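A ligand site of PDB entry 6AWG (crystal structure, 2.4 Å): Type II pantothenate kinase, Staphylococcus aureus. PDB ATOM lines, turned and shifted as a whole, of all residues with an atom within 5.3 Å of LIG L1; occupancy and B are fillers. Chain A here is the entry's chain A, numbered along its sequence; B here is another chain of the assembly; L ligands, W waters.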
ATOM      1  N   ASP A   6      -8.645 -24.239   7.282  1.00  0.00           N
ATOM      2  CA  ASP A   6      -7.883 -24.165   6.050  1.00  0.00           C
ATOM      3  C   ASP A   6      -7.283 -25.556   5.925  1.00  0.00           C
ATOM      4  O   ASP A   6      -6.375 -25.916   6.674  1.00  0.00           O
ATOM      5  CB  ASP A   6      -6.788 -23.097   6.124  1.00  0.00           C
ATOM      6  CG  ASP A   6      -5.987 -22.939   4.786  1.00  0.00           C
ATOM      7  OD1 ASP A   6      -6.348 -23.659   3.806  1.00  0.00           O
ATOM      8  OD2 ASP A   6      -4.997 -22.116   4.727  1.00  0.00           O
ATOM      9  N   GLY A   8      -5.319 -27.913   3.955  1.00  0.00           N
ATOM     10  CA  GLY A   8      -4.310 -27.849   2.923  1.00  0.00           C
ATOM     11  C   GLY A   8      -3.934 -29.233   2.464  1.00  0.00           C
ATOM     12  O   GLY A   8      -4.574 -30.230   2.830  1.00  0.00           O
ATOM     13  N   GLY A   9      -2.885 -29.280   1.662  1.00  0.00           N
ATOM     14  CA  GLY A   9      -2.406 -30.531   1.109  1.00  0.00           C
ATOM     15  C   GLY A   9      -1.785 -31.414   2.157  1.00  0.00           C
ATOM     16  O   GLY A   9      -1.816 -32.637   2.046  1.00  0.00           O
ATOM     17  N   THR A  10      -1.245 -30.783   3.198  1.00  0.00           N
ATOM     18  CA  THR A  10      -0.452 -31.491   4.231  1.00  0.00           C
ATOM     19  C   THR A  10      -1.026 -31.292   5.663  1.00  0.00           C
ATOM     20  O   THR A  10      -1.211 -32.272   6.415  1.00  0.00           O
ATOM     21  CB  THR A  10       1.030 -31.029   4.138  1.00  0.00           C
ATOM     22  OG1 THR A  10       1.473 -31.209   2.783  1.00  0.00           O
ATOM     23  CG2 THR A  10       1.919 -31.819   5.070  1.00  0.00           C
ATOM     24  N   LEU A  11      -1.290 -30.044   6.029  1.00  0.00           N
ATOM     25  CA  LEU A  11      -1.834 -29.715   7.346  1.00  0.00           C
ATOM     26  C   LEU A  11      -3.240 -29.126   7.247  1.00  0.00           C
ATOM     27  O   LEU A  11      -3.583 -28.415   6.300  1.00  0.00           O
ATOM     28  CB  LEU A  11      -0.914 -28.770   8.071  1.00  0.00           C
ATOM     29  CG  LEU A  11       0.458 -29.394   8.317  1.00  0.00           C
ATOM     30  CD1 LEU A  11       1.405 -28.334   8.861  1.00  0.00           C
ATOM     31  CD2 LEU A  11       0.447 -30.624   9.237  1.00  0.00           C
ATOM     32  N   LYS A  13      -5.504 -26.671   9.303  1.00  0.00           N
ATOM     33  CA  LYS A  13      -5.327 -25.658  10.359  1.00  0.00           C
ATOM     34  C   LYS A  13      -6.697 -25.286  10.877  1.00  0.00           C
ATOM     35  O   LYS A  13      -7.558 -24.949  10.112  1.00  0.00           O
ATOM     36  CB  LYS A  13      -4.583 -24.409   9.852  1.00  0.00           C
ATOM     37  CG  LYS A  13      -3.050 -24.562   9.789  1.00  0.00           C
ATOM     38  CD  LYS A  13      -2.591 -25.519   8.695  1.00  0.00           C
ATOM     39  CE  LYS A  13      -2.858 -24.971   7.283  1.00  0.00           C
ATOM     40  NZ  LYS A  13      -2.368 -25.825   6.201  1.00  0.00           N
ATOM     41  N   LEU A  28      -2.987 -33.366  10.755  1.00  0.00           N
ATOM     42  CA  LEU A  28      -2.608 -33.880   9.462  1.00  0.00           C
ATOM     43  C   LEU A  28      -3.793 -34.068   8.516  1.00  0.00           C
ATOM     44  O   LEU A  28      -4.832 -34.611   8.913  1.00  0.00           O
ATOM     45  CB  LEU A  28      -1.873 -35.223   9.622  1.00  0.00           C
ATOM     46  CG  LEU A  28      -0.578 -35.259  10.446  1.00  0.00           C
ATOM     47  CD1 LEU A  28       0.204 -36.531  10.119  1.00  0.00           C
ATOM     48  CD2 LEU A  28       0.293 -34.040  10.187  1.00  0.00           C
ATOM     49  N   THR A  29      -3.600 -33.608   7.273  1.00  0.00           N
ATOM     50  CA  THR A  29      -4.508 -33.880   6.151  1.00  0.00           C
ATOM     51  C   THR A  29      -4.738 -35.382   5.941  1.00  0.00           C
ATOM     52  O   THR A  29      -5.791 -35.794   5.538  1.00  0.00           O
ATOM     53  CB  THR A  29      -4.006 -33.215   4.856  1.00  0.00           C
ATOM     54  OG1 THR A  29      -3.976 -31.805   5.079  1.00  0.00           O
ATOM     55  CG2 THR A  29      -4.918 -33.497   3.651  1.00  0.00           C
ATOM     56  N   GLU A  70      -8.878 -19.781  -0.958  1.00  0.00           N
ATOM     57  CA  GLU A  70      -7.777 -19.670   0.013  1.00  0.00           C
ATOM     58  C   GLU A  70      -6.881 -18.439  -0.141  1.00  0.00           C
ATOM     59  O   GLU A  70      -6.242 -18.031   0.839  1.00  0.00           O
ATOM     60  CB  GLU A  70      -6.912 -20.935   0.024  1.00  0.00           C
ATOM     61  CG  GLU A  70      -6.126 -21.203  -1.252  1.00  0.00           C
ATOM     62  CD  GLU A  70      -5.077 -22.300  -1.063  1.00  0.00           C
ATOM     63  OE1 GLU A  70      -4.008 -22.007  -0.482  1.00  0.00           O
ATOM     64  OE2 GLU A  70      -5.324 -23.445  -1.502  1.00  0.00           O
ATOM     65  N   ASN A  96       3.128 -17.527   0.713  1.00  0.00           N
ATOM     66  CA  ASN A  96       2.498 -18.561   1.520  1.00  0.00           C
ATOM     67  C   ASN A  96       3.279 -19.846   1.190  1.00  0.00           C
ATOM     68  O   ASN A  96       3.013 -20.514   0.159  1.00  0.00           O
ATOM     69  CB  ASN A  96       1.007 -18.670   1.189  1.00  0.00           C
ATOM     70  CG  ASN A  96       0.264 -19.592   2.134  1.00  0.00           C
ATOM     71  OD1 ASN A  96       0.863 -20.313   2.912  1.00  0.00           O
ATOM     72  ND2 ASN A  96      -1.058 -19.579   2.073  1.00  0.00           N
ATOM     73  N   VAL A  97       4.239 -20.149   2.053  1.00  0.00           N
ATOM     74  CA  VAL A  97       5.167 -21.274   1.859  1.00  0.00           C
ATOM     75  C   VAL A  97       4.561 -22.527   2.485  1.00  0.00           C
ATOM     76  O   VAL A  97       4.834 -22.895   3.599  1.00  0.00           O
ATOM     77  CB  VAL A  97       6.578 -20.943   2.372  1.00  0.00           C
ATOM     78  CG1 VAL A  97       7.589 -21.989   1.907  1.00  0.00           C
ATOM     79  CG2 VAL A  97       7.037 -19.575   1.916  1.00  0.00           C
ATOM     80  N   GLY A  98       3.682 -23.165   1.735  1.00  0.00           N
ATOM     81  CA  GLY A  98       3.028 -24.342   2.204  1.00  0.00           C
ATOM     82  C   GLY A  98       3.607 -25.564   1.604  1.00  0.00           C
ATOM     83  O   GLY A  98       4.806 -25.694   1.489  1.00  0.00           O
ATOM     84  N   THR A  99       2.763 -26.503   1.259  1.00  0.00           N
ATOM     85  CA  THR A  99       3.221 -27.677   0.527  1.00  0.00           C
ATOM     86  C   THR A  99       3.896 -27.209  -0.772  1.00  0.00           C
ATOM     87  O   THR A  99       4.976 -27.704  -1.129  1.00  0.00           O
ATOM     88  CB  THR A  99       2.040 -28.592   0.222  1.00  0.00           C
ATOM     89  OG1 THR A  99       1.434 -28.993   1.483  1.00  0.00           O
ATOM     90  CG2 THR A  99       2.500 -29.804  -0.569  1.00  0.00           C
ATOM     91  N   GLY A 100       3.235 -26.271  -1.450  1.00  0.00           N
ATOM     92  CA  GLY A 100       3.794 -25.454  -2.498  1.00  0.00           C
ATOM     93  C   GLY A 100       3.766 -23.988  -2.037  1.00  0.00           C
ATOM     94  O   GLY A 100       3.239 -23.697  -0.954  1.00  0.00           O
ATOM     95  N   GLY A 121       7.433 -26.590   1.342  1.00  0.00           N
ATOM     96  CA  GLY A 121       7.587 -27.669   2.334  1.00  0.00           C
ATOM     97  C   GLY A 121       7.459 -29.106   1.809  1.00  0.00           C
ATOM     98  O   GLY A 121       8.103 -30.025   2.338  1.00  0.00           O
ATOM     99  N   GLY A 122       6.654 -29.296   0.766  1.00  0.00           N
ATOM    100  CA  GLY A 122       6.500 -30.594   0.118  1.00  0.00           C
ATOM    101  C   GLY A 122       7.820 -31.030  -0.424  1.00  0.00           C
ATOM    102  O   GLY A 122       8.209 -32.180  -0.289  1.00  0.00           O
ATOM    103  N   ILE A 124      10.697 -30.139   0.734  1.00  0.00           N
ATOM    104  CA  ILE A 124      11.588 -30.363   1.871  1.00  0.00           C
ATOM    105  C   ILE A 124      11.391 -31.767   2.409  1.00  0.00           C
ATOM    106  O   ILE A 124      12.356 -32.500   2.667  1.00  0.00           O
ATOM    107  CB  ILE A 124      11.379 -29.313   2.961  1.00  0.00           C
ATOM    108  CG1 ILE A 124      11.807 -27.936   2.415  1.00  0.00           C
ATOM    109  CG2 ILE A 124      12.201 -29.634   4.211  1.00  0.00           C
ATOM    110  CD1 ILE A 124      11.469 -26.725   3.255  1.00  0.00           C
ATOM    111  N   GLN A 125      10.127 -32.122   2.543  1.00  0.00           N
ATOM    112  CA  GLN A 125       9.730 -33.486   2.918  1.00  0.00           C
ATOM    113  C   GLN A 125      10.054 -34.548   1.895  1.00  0.00           C
ATOM    114  O   GLN A 125      10.551 -35.602   2.243  1.00  0.00           O
ATOM    115  CB  GLN A 125       8.237 -33.522   3.195  1.00  0.00           C
ATOM    116  CG  GLN A 125       7.823 -32.647   4.352  1.00  0.00           C
ATOM    117  CD  GLN A 125       6.415 -32.969   4.803  1.00  0.00           C
ATOM    118  OE1 GLN A 125       5.435 -32.340   4.358  1.00  0.00           O
ATOM    119  NE2 GLN A 125       6.308 -33.983   5.648  1.00  0.00           N
ATOM    120  N   TYR A 137       8.693 -35.545  10.150  1.00  0.00           N
ATOM    121  CA  TYR A 137       8.998 -34.131   9.858  1.00  0.00           C
ATOM    122  C   TYR A 137       9.945 -33.473  10.889  1.00  0.00           C
ATOM    123  O   TYR A 137      10.850 -32.692  10.524  1.00  0.00           O
ATOM    124  CB  TYR A 137       7.713 -33.303   9.738  1.00  0.00           C
ATOM    125  CG  TYR A 137       7.978 -31.804   9.506  1.00  0.00           C
ATOM    126  CD1 TYR A 137       8.308 -31.318   8.246  1.00  0.00           C
ATOM    127  CD2 TYR A 137       7.927 -30.879  10.567  1.00  0.00           C
ATOM    128  CE1 TYR A 137       8.524 -29.971   8.034  1.00  0.00           C
ATOM    129  CE2 TYR A 137       8.173 -29.521  10.357  1.00  0.00           C
ATOM    130  CZ  TYR A 137       8.478 -29.067   9.090  1.00  0.00           C
ATOM    131  OH  TYR A 137       8.736 -27.718   8.847  1.00  0.00           O
ATOM    132  N   GLY A 224       3.072 -19.674   6.255  1.00  0.00           N
ATOM    133  CA  GLY A 224       2.988 -21.099   5.957  1.00  0.00           C
ATOM    134  C   GLY A 224       3.688 -21.852   7.074  1.00  0.00           C
ATOM    135  O   GLY A 224       4.530 -21.294   7.808  1.00  0.00           O
ATOM    136  N   SER A 225       3.355 -23.119   7.203  1.00  0.00           N
ATOM    137  CA  SER A 225       3.842 -23.932   8.259  1.00  0.00           C
ATOM    138  C   SER A 225       5.276 -24.390   8.007  1.00  0.00           C
ATOM    139  O   SER A 225       5.908 -24.874   8.917  1.00  0.00           O
ATOM    140  CB  SER A 225       2.953 -25.157   8.414  1.00  0.00           C
ATOM    141  OG  SER A 225       1.626 -24.731   8.565  1.00  0.00           O
ATOM    142  N   SER A 226       5.760 -24.247   6.784  1.00  0.00           N
ATOM    143  CA  SER A 226       7.099 -24.688   6.394  1.00  0.00           C
ATOM    144  C   SER A 226       8.205 -24.096   7.255  1.00  0.00           C
ATOM    145  O   SER A 226       9.305 -24.663   7.291  1.00  0.00           O
ATOM    146  CB  SER A 226       7.367 -24.337   4.911  1.00  0.00           C
ATOM    147  OG  SER A 226       6.530 -25.102   4.060  1.00  0.00           O
ATOM    148  N   HIS A 228       7.829 -23.684  10.644  1.00  0.00           N
ATOM    149  CA  HIS A 228       7.673 -24.242  11.988  1.00  0.00           C
ATOM    150  C   HIS A 228       8.684 -25.309  12.194  1.00  0.00           C
ATOM    151  O   HIS A 228       8.785 -26.231  11.369  1.00  0.00           O
ATOM    152  CB  HIS A 228       6.302 -24.866  12.209  1.00  0.00           C
ATOM    153  CG  HIS A 228       5.166 -23.889  12.108  1.00  0.00           C
ATOM    154  ND1 HIS A 228       3.841 -24.288  12.039  1.00  0.00           N
ATOM    155  CD2 HIS A 228       5.154 -22.530  12.045  1.00  0.00           C
ATOM    156  CE1 HIS A 228       3.070 -23.222  11.963  1.00  0.00           C
ATOM    157  NE2 HIS A 228       3.830 -22.142  11.962  1.00  0.00           N
ATOM    158  N   ILE B 159      -4.047 -31.712  -4.631  1.00  0.00           N
ATOM    159  CA  ILE B 159      -4.365 -31.058  -3.370  1.00  0.00           C
ATOM    160  C   ILE B 159      -5.880 -30.777  -3.340  1.00  0.00           C
ATOM    161  O   ILE B 159      -6.559 -31.036  -2.333  1.00  0.00           O
ATOM    162  CB  ILE B 159      -3.566 -29.773  -3.194  1.00  0.00           C
ATOM    163  CG1 ILE B 159      -2.061 -30.133  -3.087  1.00  0.00           C
ATOM    164  CG2 ILE B 159      -4.020 -29.043  -1.955  1.00  0.00           C
ATOM    165  CD1 ILE B 159      -1.124 -28.942  -2.974  1.00  0.00           C
HETATM  166  P1  LIG L   1      -1.072 -25.896   0.469  1.00  0.00           P
HETATM  167  O1  LIG L   1       0.143 -25.429  -0.398  1.00  0.00           O
HETATM  168  O2  LIG L   1      -2.117 -26.869  -0.066  1.00  0.00           O
HETATM  169  O3  LIG L   1      -1.804 -24.737   1.128  1.00  0.00           O
HETATM  170  P2  LIG L   1      -0.708 -26.640   3.219  1.00  0.00           P
HETATM  171  O4  LIG L   1      -1.681 -25.508   3.334  1.00  0.00           O
HETATM  172  O5  LIG L   1      -0.941 -27.992   3.799  1.00  0.00           O
HETATM  173  O6  LIG L   1      -0.388 -26.773   1.661  1.00  0.00           O
HETATM  174  P3  LIG L   1       1.159 -25.566   5.136  1.00  0.00           P
HETATM  175  O7  LIG L   1       1.265 -24.097   4.911  1.00  0.00           O
HETATM  176  O8  LIG L   1       0.344 -25.968   6.328  1.00  0.00           O
HETATM  177  O9  LIG L   1       0.721 -26.184   3.718  1.00  0.00           O
HETATM  178  O10 LIG L   1       2.673 -26.072   5.272  1.00  0.00           O
HETATM  179  C1  LIG L   1       3.001 -27.369   4.833  1.00  0.00           C
HETATM  180  C2  LIG L   1       4.434 -27.701   5.244  1.00  0.00           C
HETATM  181  O11 LIG L   1       4.602 -27.447   6.617  1.00  0.00           O
HETATM  182  C3  LIG L   1       4.801 -29.163   5.147  1.00  0.00           C
HETATM  183  O12 LIG L   1       5.055 -29.630   3.825  1.00  0.00           O
HETATM  184  C4  LIG L   1       6.047 -29.208   6.001  1.00  0.00           C
HETATM  185  O13 LIG L   1       7.219 -28.804   5.306  1.00  0.00           O
HETATM  186  C5  LIG L   1       5.712 -28.209   7.082  1.00  0.00           C
HETATM  187  N1  LIG L   1       5.293 -28.825   8.346  1.00  0.00           N
HETATM  188  C6  LIG L   1       5.230 -28.146   9.507  1.00  0.00           C
HETATM  189  N2  LIG L   1       4.809 -28.971  10.459  1.00  0.00           N
HETATM  190  C7  LIG L   1       4.604 -30.168   9.936  1.00  0.00           C
HETATM  191  C8  LIG L   1       4.160 -31.463  10.419  1.00  0.00           C
HETATM  192  N3  LIG L   1       3.859 -31.575  11.718  1.00  0.00           N
HETATM  193  N4  LIG L   1       4.051 -32.507   9.580  1.00  0.00           N
HETATM  194  C9  LIG L   1       4.349 -32.362   8.297  1.00  0.00           C
HETATM  195  N5  LIG L   1       4.738 -31.191   7.809  1.00  0.00           N
HETATM  196  C10 LIG L   1       4.908 -30.074   8.551  1.00  0.00           C
HETATM  197  C1  LG2 L   2      -2.209 -24.809  -2.975  1.00  0.00           C
HETATM  198  C2  LG2 L   2      -1.493 -24.096  -4.150  1.00  0.00           C
HETATM  199  C3  LG2 L   2      -2.236 -22.751  -4.350  1.00  0.00           C
HETATM  200  C4  LG2 L   2      -1.568 -24.917  -5.432  1.00  0.00           C
HETATM  201  C5  LG2 L   2       0.022 -23.897  -3.779  1.00  0.00           C
HETATM  202  O1  LG2 L   2       0.686 -25.116  -3.315  1.00  0.00           O
HETATM  203  C6  LG2 L   2       0.822 -23.272  -4.954  1.00  0.00           C
HETATM  204  O2  LG2 L   2       0.676 -22.109  -5.293  1.00  0.00           O
HETATM  205  N1  LG2 L   2       1.693 -24.114  -5.495  1.00  0.00           N
HETATM  206  C7  LG2 L   2       2.594 -23.741  -6.593  1.00  0.00           C
HETATM  207  C8  LG2 L   2       1.788 -23.768  -7.888  1.00  0.00           C
HETATM  208  C9  LG2 L   2       2.573 -23.034  -8.957  1.00  0.00           C
HETATM  209  O3  LG2 L   2       2.350 -21.844  -9.116  1.00  0.00           O
HETATM  210  N2  LG2 L   2       3.492 -23.756  -9.668  1.00  0.00           N
HETATM  211  C10 LG2 L   2       4.300 -23.108 -10.684  1.00  0.00           C
HETATM  212  C11 LG2 L   2       4.615 -23.913 -11.815  1.00  0.00           C
HETATM  213  C12 LG2 L   2       3.809 -24.933 -12.311  1.00  0.00           C
HETATM  214  C13 LG2 L   2       4.158 -25.609 -13.414  1.00  0.00           C
HETATM  215  O4  LG2 L   2       3.484 -26.609 -14.031  1.00  0.00           O
HETATM  216  C14 LG2 L   2       4.382 -27.072 -15.024  1.00  0.00           C
HETATM  217  O5  LG2 L   2       5.434 -26.106 -15.135  1.00  0.00           O
HETATM  218  C15 LG2 L   2       5.279 -25.310 -14.070  1.00  0.00           C
HETATM  219  C16 LG2 L   2       6.070 -24.350 -13.658  1.00  0.00           C
HETATM  220  C17 LG2 L   2       5.754 -23.622 -12.544  1.00  0.00           C
HETATM  221  O   HOH W   1       0.535 -22.507  -0.281  1.00  0.00           O
HETATM  222  O   HOH W   2      -4.265 -24.266   2.296  1.00  0.00           O
HETATM  223  O   HOH W   3      -4.963 -25.612  -0.043  1.00  0.00           O
HETATM  224  O   HOH W   4       0.144 -22.638   2.868  1.00  0.00           O
HETATM  225  O   HOH W   5      -0.396 -22.441   6.182  1.00  0.00           O
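The side-chain amino group (NZ) of Lys 13 is in salt-bridge range of an oxygen (O8) of LIG L1, at 2.7 Å. The side-chain amide oxygen of Gln 125 sits at hydrogen-bond distance from an oxygen (O12) of LIG L1, 2.8 Å away. An oxygen (O7) of LIG L1 is in hydrogen-bond range of the backbone NH (N) of Ser 225 (3.3 Å). OG of Ser 225 sits at hydrogen-bond distance from O8 of LIG L1. The backbone NH (N) of Thr 10 is in hydrogen-bond range of an oxygen (O5) of LIG L1 (2.9 Å). The backbone NH (N) of Thr 99 sits at hydrogen-bond distance from an oxygen (O6) of LIG L1. OG1 of Thr 99 sits at hydrogen-bond distance from O6 of LIG L1 (2.9 Å). O5 of LIG L1 lies within hydrogen-bond range of N of Leu 11 (3.1 Å). The backbone NH (N) of Gly 9 sits at hydrogen-bond distance from an oxygen (O2) of LIG L1. An oxygen (O13) of LIG L1 sits close to the backbone carbonyl oxygen (O) of Gly 121, at 3.3 Å. The backbone NH of Gly 100 is in hydrogen-bond range of an oxygen (O1) of LIG L1 (3.4 Å). The backbone NH (N) of Ser 226 sits at hydrogen-bond distance from an oxygen (O11) of LIG L1 (3.4 Å). The backbone NH of Gly 122 lies within hydrogen-bond range of an oxygen (O12) of LIG L1, 3.5 Å away. An oxygen (O1) of LG2 L2 sits close to the backbone NH of Gly 100 (3.4 Å).
An oxygen (O1) of LG2 L2 lies within hydrogen-bond range of an oxygen (O1) of LIG L1, at 3.0 Å.
The backbone NH (N) of Lys 13 lies within hydrogen-bond range of the backbone carbonyl oxygen (O) of Asp 6 (2.9 Å). The side-chain hydroxyl (OG1) of Thr 99 lies within hydrogen-bond range of the side-chain hydroxyl (OG1) of Thr 10, 2.6 Å away. The backbone NH of Thr 29 lies within hydrogen-bond range of the backbone carbonyl oxygen of Thr 10, at 2.9 Å. The backbone NH of Leu 11 is in hydrogen-bond range of the side-chain hydroxyl of Thr 29, at 3.3 Å. The backbone NH of Gly 121 is in hydrogen-bond range of the side-chain hydroxyl of Ser 226. O of His 228 lies within hydrogen-bond range of OH of Tyr 137 (2.9 Å). OG of Ser 226 lies within hydrogen-bond range of O of Val 97 (2.8 Å). The backbone carbonyl oxygen (O) of Gly 8 is in hydrogen-bond range of the side-chain hydroxyl (OG1) of Thr 29 (2.8 Å).
Merely in contact with LIG L1: Gly 98 (3.2 Å), Tyr 137 (3.2 Å), Ile 159 of chain B (3.5 Å), Gly 8 (3.5 Å), Gly 224 (3.6 Å), Glu 70 (3.9 Å) and Val 97 (3.99 Å). Hydrophobic or aromatic side chains within 4 Å of LIG L1: Leu 11, Tyr 137 and Ile 159 of chain B. Of the 24 residues printed, 18 come within 4 Å of LIG L1.
Water W4 bridges the side-chain amide oxygen (OD1) of Asn 96 (2.4 Å) and an oxygen (O7) of LIG L1 (2.7 Å). Water W2 lies within hydrogen-bond range of OD1 of Asp 6 (2.6 Å) and O3 of LIG L1 (2.8 Å). Water W1 lies within hydrogen-bond range of O1 of LIG L1, O of Gly 100 and O of Asn 96. Water W3 bridges OE2 of Glu 70 (2.6 Å) and O2 of LIG L1 (3.1 Å).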
